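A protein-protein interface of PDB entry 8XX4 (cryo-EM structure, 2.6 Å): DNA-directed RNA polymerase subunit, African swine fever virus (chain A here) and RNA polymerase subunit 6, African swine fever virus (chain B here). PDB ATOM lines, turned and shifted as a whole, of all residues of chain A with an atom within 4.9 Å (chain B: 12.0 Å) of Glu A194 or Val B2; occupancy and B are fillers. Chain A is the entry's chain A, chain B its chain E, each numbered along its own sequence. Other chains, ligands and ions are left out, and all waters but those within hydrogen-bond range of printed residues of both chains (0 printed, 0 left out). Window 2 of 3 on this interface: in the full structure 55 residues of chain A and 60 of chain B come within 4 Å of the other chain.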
ATOM      1  N   ARG A 171      35.363 -12.155  20.267  1.00  0.00           N
ATOM      2  CA  ARG A 171      34.359 -11.633  21.186  1.00  0.00           C
ATOM      3  C   ARG A 171      34.431 -10.116  21.270  1.00  0.00           C
ATOM      4  O   ARG A 171      33.398  -9.441  21.250  1.00  0.00           O
ATOM      5  CB  ARG A 171      34.536 -12.261  22.568  1.00  0.00           C
ATOM      6  CG  ARG A 171      34.008 -11.430  23.724  1.00  0.00           C
ATOM      7  CD  ARG A 171      32.490 -11.363  23.732  1.00  0.00           C
ATOM      8  NE  ARG A 171      31.876 -12.514  24.383  1.00  0.00           N
ATOM      9  CZ  ARG A 171      31.893 -12.741  25.689  1.00  0.00           C
ATOM     10  NH1 ARG A 171      32.508 -11.921  26.526  1.00  0.00           N
ATOM     11  NH2 ARG A 171      31.275 -13.815  26.169  1.00  0.00           N
ATOM     12  N   PHE A 174      33.136  -8.613  17.933  1.00  0.00           N
ATOM     13  CA  PHE A 174      31.685  -8.695  17.841  1.00  0.00           C
ATOM     14  C   PHE A 174      31.005  -7.797  18.861  1.00  0.00           C
ATOM     15  O   PHE A 174      29.896  -7.315  18.614  1.00  0.00           O
ATOM     16  CB  PHE A 174      31.242 -10.142  18.018  1.00  0.00           C
ATOM     17  CG  PHE A 174      31.497 -10.996  16.817  1.00  0.00           C
ATOM     18  CD1 PHE A 174      31.770 -10.421  15.594  1.00  0.00           C
ATOM     19  CD2 PHE A 174      31.466 -12.372  16.910  1.00  0.00           C
ATOM     20  CE1 PHE A 174      32.003 -11.197  14.490  1.00  0.00           C
ATOM     21  CE2 PHE A 174      31.694 -13.152  15.805  1.00  0.00           C
ATOM     22  CZ  PHE A 174      31.967 -12.564  14.595  1.00  0.00           C
ATOM     23  N   SER A 175      31.646  -7.560  20.005  1.00  0.00           N
ATOM     24  CA  SER A 175      31.075  -6.664  21.000  1.00  0.00           C
ATOM     25  C   SER A 175      31.078  -5.225  20.513  1.00  0.00           C
ATOM     26  O   SER A 175      30.206  -4.441  20.901  1.00  0.00           O
ATOM     27  CB  SER A 175      31.847  -6.779  22.309  1.00  0.00           C
ATOM     28  OG  SER A 175      33.097  -6.125  22.213  1.00  0.00           O
ATOM     29  N   VAL A 177      30.206  -4.314  17.688  1.00  0.00           N
ATOM     30  CA  VAL A 177      29.131  -4.163  16.714  1.00  0.00           C
ATOM     31  C   VAL A 177      27.899  -3.598  17.405  1.00  0.00           C
ATOM     32  O   VAL A 177      27.518  -4.048  18.492  1.00  0.00           O
ATOM     33  CB  VAL A 177      28.811  -5.506  16.040  1.00  0.00           C
ATOM     34  CG1 VAL A 177      27.843  -5.304  14.894  1.00  0.00           C
ATOM     35  CG2 VAL A 177      30.071  -6.168  15.560  1.00  0.00           C
ATOM     36  N   THR A 178      27.269  -2.615  16.775  1.00  0.00           N
ATOM     37  CA  THR A 178      26.048  -2.026  17.299  1.00  0.00           C
ATOM     38  C   THR A 178      24.836  -2.862  16.901  1.00  0.00           C
ATOM     39  O   THR A 178      24.883  -3.671  15.973  1.00  0.00           O
ATOM     40  CB  THR A 178      25.880  -0.594  16.794  1.00  0.00           C
ATOM     41  OG1 THR A 178      26.432  -0.485  15.477  1.00  0.00           O
ATOM     42  CG2 THR A 178      26.591   0.378  17.714  1.00  0.00           C
ATOM     43  N   TYR A 179      23.736  -2.654  17.629  1.00  0.00           N
ATOM     44  CA  TYR A 179      22.486  -3.326  17.287  1.00  0.00           C
ATOM     45  C   TYR A 179      21.938  -2.845  15.953  1.00  0.00           C
ATOM     46  O   TYR A 179      21.222  -3.589  15.275  1.00  0.00           O
ATOM     47  CB  TYR A 179      21.456  -3.108  18.393  1.00  0.00           C
ATOM     48  CG  TYR A 179      21.617  -4.045  19.562  1.00  0.00           C
ATOM     49  CD1 TYR A 179      21.800  -5.405  19.362  1.00  0.00           C
ATOM     50  CD2 TYR A 179      21.565  -3.577  20.865  1.00  0.00           C
ATOM     51  CE1 TYR A 179      21.940  -6.265  20.423  1.00  0.00           C
ATOM     52  CE2 TYR A 179      21.708  -4.433  21.933  1.00  0.00           C
ATOM     53  CZ  TYR A 179      21.894  -5.777  21.705  1.00  0.00           C
ATOM     54  OH  TYR A 179      22.037  -6.640  22.766  1.00  0.00           O
ATOM     55  N   HIS A 192      22.575 -11.189  17.992  1.00  0.00           N
ATOM     56  CA  HIS A 192      23.786 -10.388  17.946  1.00  0.00           C
ATOM     57  C   HIS A 192      25.007 -11.302  17.880  1.00  0.00           C
ATOM     58  O   HIS A 192      25.038 -12.344  18.544  1.00  0.00           O
ATOM     59  CB  HIS A 192      23.867  -9.485  19.177  1.00  0.00           C
ATOM     60  CG  HIS A 192      24.894  -8.402  19.073  1.00  0.00           C
ATOM     61  ND1 HIS A 192      26.241  -8.635  19.246  1.00  0.00           N
ATOM     62  CD2 HIS A 192      24.772  -7.077  18.827  1.00  0.00           C
ATOM     63  CE1 HIS A 192      26.905  -7.503  19.103  1.00  0.00           C
ATOM     64  NE2 HIS A 192      26.037  -6.542  18.848  1.00  0.00           N
ATOM     65  N   PRO A 193      26.024 -10.954  17.089  1.00  0.00           N
ATOM     66  CA  PRO A 193      27.193 -11.838  16.969  1.00  0.00           C
ATOM     67  C   PRO A 193      27.961 -12.020  18.262  1.00  0.00           C
ATOM     68  O   PRO A 193      28.768 -12.952  18.355  1.00  0.00           O
ATOM     69  CB  PRO A 193      28.048 -11.147  15.900  1.00  0.00           C
ATOM     70  CG  PRO A 193      27.581  -9.744  15.882  1.00  0.00           C
ATOM     71  CD  PRO A 193      26.122  -9.799  16.185  1.00  0.00           C
ATOM     72  N   GLU A 194      27.752 -11.160  19.260  1.00  0.00           N
ATOM     73  CA  GLU A 194      28.435 -11.334  20.536  1.00  0.00           C
ATOM     74  C   GLU A 194      28.044 -12.646  21.203  1.00  0.00           C
ATOM     75  O   GLU A 194      28.847 -13.230  21.937  1.00  0.00           O
ATOM     76  CB  GLU A 194      28.130 -10.156  21.457  1.00  0.00           C
ATOM     77  CG  GLU A 194      28.914 -10.161  22.751  1.00  0.00           C
ATOM     78  CD  GLU A 194      28.042 -10.454  23.953  1.00  0.00           C
ATOM     79  OE1 GLU A 194      28.544 -11.069  24.919  1.00  0.00           O
ATOM     80  OE2 GLU A 194      26.854 -10.071  23.931  1.00  0.00           O
ATOM     81  N   LYS A 195      26.825 -13.129  20.950  1.00  0.00           N
ATOM     82  CA  LYS A 195      26.387 -14.406  21.498  1.00  0.00           C
ATOM     83  C   LYS A 195      27.193 -15.577  20.955  1.00  0.00           C
ATOM     84  O   LYS A 195      27.189 -16.652  21.563  1.00  0.00           O
ATOM     85  CB  LYS A 195      24.909 -14.633  21.187  1.00  0.00           C
ATOM     86  CG  LYS A 195      23.957 -13.713  21.912  1.00  0.00           C
ATOM     87  CD  LYS A 195      22.547 -14.266  21.860  1.00  0.00           C
ATOM     88  CE  LYS A 195      21.548 -13.289  22.437  1.00  0.00           C
ATOM     89  NZ  LYS A 195      20.917 -13.824  23.668  1.00  0.00           N
ATOM     90  N   LEU A 196      27.876 -15.397  19.826  1.00  0.00           N
ATOM     91  CA  LEU A 196      28.564 -16.498  19.169  1.00  0.00           C
ATOM     92  C   LEU A 196      29.857 -16.897  19.862  1.00  0.00           C
ATOM     93  O   LEU A 196      30.450 -17.911  19.484  1.00  0.00           O
ATOM     94  CB  LEU A 196      28.845 -16.135  17.716  1.00  0.00           C
ATOM     95  CG  LEU A 196      27.616 -15.713  16.914  1.00  0.00           C
ATOM     96  CD1 LEU A 196      28.015 -15.192  15.547  1.00  0.00           C
ATOM     97  CD2 LEU A 196      26.653 -16.873  16.790  1.00  0.00           C
ATOM     98  N   VAL A 197      30.310 -16.136  20.852  1.00  0.00           N
ATOM     99  CA  VAL A 197      31.490 -16.477  21.638  1.00  0.00           C
ATOM    100  C   VAL A 197      31.033 -16.745  23.062  1.00  0.00           C
ATOM    101  O   VAL A 197      30.426 -15.879  23.702  1.00  0.00           O
ATOM    102  CB  VAL A 197      32.547 -15.366  21.593  1.00  0.00           C
ATOM    103  CG1 VAL A 197      33.754 -15.769  22.405  1.00  0.00           C
ATOM    104  CG2 VAL A 197      32.946 -15.076  20.162  1.00  0.00           C
ATOM    105  N   ILE B   1      30.292  -0.831  24.101  1.00  0.00           N
ATOM    106  CA  ILE B   1      30.305  -2.287  24.066  1.00  0.00           C
ATOM    107  C   ILE B   1      28.894  -2.831  24.258  1.00  0.00           C
ATOM    108  O   ILE B   1      28.060  -2.207  24.915  1.00  0.00           O
ATOM    109  CB  ILE B   1      31.269  -2.855  25.120  1.00  0.00           C
ATOM    110  CG1 ILE B   1      30.804  -2.491  26.532  1.00  0.00           C
ATOM    111  CG2 ILE B   1      32.680  -2.345  24.875  1.00  0.00           C
ATOM    112  CD1 ILE B   1      30.338  -3.674  27.352  1.00  0.00           C
ATOM    113  N   VAL B   2      28.628  -3.998  23.676  1.00  0.00           N
ATOM    114  CA  VAL B   2      27.311  -4.620  23.713  1.00  0.00           C
ATOM    115  C   VAL B   2      27.430  -5.968  24.408  1.00  0.00           C
ATOM    116  O   VAL B   2      28.290  -6.782  24.053  1.00  0.00           O
ATOM    117  CB  VAL B   2      26.723  -4.785  22.300  1.00  0.00           C
ATOM    118  CG1 VAL B   2      25.388  -5.506  22.363  1.00  0.00           C
ATOM    119  CG2 VAL B   2      26.579  -3.436  21.624  1.00  0.00           C
ATOM    120  N   GLU B   3      26.574  -6.196  25.403  1.00  0.00           N
ATOM    121  CA  GLU B   3      26.486  -7.471  26.107  1.00  0.00           C
ATOM    122  C   GLU B   3      25.054  -7.972  25.980  1.00  0.00           C
ATOM    123  O   GLU B   3      24.127  -7.362  26.525  1.00  0.00           O
ATOM    124  CB  GLU B   3      26.893  -7.328  27.571  1.00  0.00           C
ATOM    125  CG  GLU B   3      27.058  -8.654  28.294  1.00  0.00           C
ATOM    126  CD  GLU B   3      26.013  -8.861  29.370  1.00  0.00           C
ATOM    127  OE1 GLU B   3      25.003  -8.124  29.367  1.00  0.00           O
ATOM    128  OE2 GLU B   3      26.197  -9.756  30.219  1.00  0.00           O
ATOM    129  N   SER B   4      24.880  -9.079  25.274  1.00  0.00           N
ATOM    130  CA  SER B   4      23.545  -9.539  24.910  1.00  0.00           C
ATOM    131  C   SER B   4      22.784 -10.021  26.139  1.00  0.00           C
ATOM    132  O   SER B   4      23.274 -10.894  26.862  1.00  0.00           O
ATOM    133  CB  SER B   4      23.646 -10.661  23.892  1.00  0.00           C
ATOM    134  OG  SER B   4      24.196 -11.816  24.495  1.00  0.00           O
ATOM    135  N   PRO B   5      21.593  -9.491  26.404  1.00  0.00           N
ATOM    136  CA  PRO B   5      20.779 -10.005  27.508  1.00  0.00           C
ATOM    137  C   PRO B   5      20.185 -11.362  27.167  1.00  0.00           C
ATOM    138  O   PRO B   5      20.197 -11.814  26.020  1.00  0.00           O
ATOM    139  CB  PRO B   5      19.692  -8.941  27.667  1.00  0.00           C
ATOM    140  CG  PRO B   5      19.560  -8.365  26.299  1.00  0.00           C
ATOM    141  CD  PRO B   5      20.963  -8.326  25.759  1.00  0.00           C
ATOM    142  N   SER B   6      19.658 -12.017  28.196  1.00  0.00           N
ATOM    143  CA  SER B   6      19.025 -13.311  28.010  1.00  0.00           C
ATOM    144  C   SER B   6      17.758 -13.172  27.174  1.00  0.00           C
ATOM    145  O   SER B   6      17.134 -12.111  27.111  1.00  0.00           O
ATOM    146  CB  SER B   6      18.702 -13.951  29.358  1.00  0.00           C
ATOM    147  OG  SER B   6      18.373 -12.970  30.325  1.00  0.00           O
ATOM    148  N   ILE B   7      17.392 -14.270  26.509  1.00  0.00           N
ATOM    149  CA  ILE B   7      16.201 -14.266  25.667  1.00  0.00           C
ATOM    150  C   ILE B   7      14.949 -14.063  26.509  1.00  0.00           C
ATOM    151  O   ILE B   7      13.999 -13.399  26.079  1.00  0.00           O
ATOM    152  CB  ILE B   7      16.119 -15.567  24.852  1.00  0.00           C
ATOM    153  CG1 ILE B   7      17.464 -15.877  24.200  1.00  0.00           C
ATOM    154  CG2 ILE B   7      15.017 -15.470  23.813  1.00  0.00           C
ATOM    155  CD1 ILE B   7      17.842 -14.918  23.114  1.00  0.00           C
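N of Val B2 sits at hydrogen-bond distance from O of Ser A175 (3.2 Å).
OE2 of Glu A194 is in hydrogen-bond range of N of Ser B4 (2.6 Å).
The side-chain amino group (NZ) of Lys A195 lies within hydrogen-bond range of the backbone carbonyl oxygen (O) of Pro B5.
O of Arg A171 lies close to OG of Ser A175 (3.5 Å).
The guanidinium group (NE) of Arg A171 is in salt-bridge range of the side-chain carboxylate (OE1) of Glu A194 (3.7 Å).
The backbone carbonyl oxygen of Val A177 is in hydrogen-bond range of a ring nitrogen (NE2) of His A192.
A ring nitrogen (ND1) of His A192 lies within hydrogen-bond range of the backbone NH (N) of Glu A194 (2.9 Å).
Among the printed residues, pairs that only touch across the chains: Lys A195 with Ser B4, Lys A195 with Ile B7, Val A177 with Val B2, Glu A194 with Glu B3, Tyr A179 with Val B2, Glu A194 with Val B2, Tyr A179 with Pro B5, His A192 with Val B2, Ser A175 with Ile B1 and Tyr A179 with Ser B4.
Of chain B, only Val B2, Glu B3 and Ser B4 come within 4 Å of Glu A194.
Of chain A, only Ser A175, Val A177, Tyr A179, His A192 and Glu A194 come within 4 Å of Val B2.
Arg A171 touches none of the printed residues of chain B.
Of chain B, only Ile B1 and Val B2 come within 4 Å of Ser A175.
Val A177 touches just one residue of chain B: Val B2.
No residue of chain B comes within 4 Å of Thr A178.
His A192 touches just one residue of chain B: Val B2 (3.7 Å).
No residue of chain B comes within 4 Å of Pro A193.
No residue of chain B comes within 4 Å of Val A197.
Printed residues of chain A within 4 Å of Ile B1: Ser A175 (3.8 Å).
Of the printed residues of chain A, Ile B7 touches Lys A195 (3.3 Å).
Ser B6 touches none of the printed residues of chain A.
The nearest residue of chain B that does not touch Glu A194 is Pro B5 (5.8 Å).
The nearest printed residue of chain B that does not touch Tyr A179 is Glu B3 (4.4 Å).
Hydrophobic or aromatic side chains of chain A within 4 Å of the printed part of chain B: Tyr A179 and His A192.
Along chain A the printed residues that touch a printed residue of chain B span positions 175 to 195.
Among the printed residues, 13 pairs touch across the chains.
Among the printed residues, no Asp or Glu carboxylate lies within 4 Å of a Lys or Arg side-chain nitrogen of the other chain.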
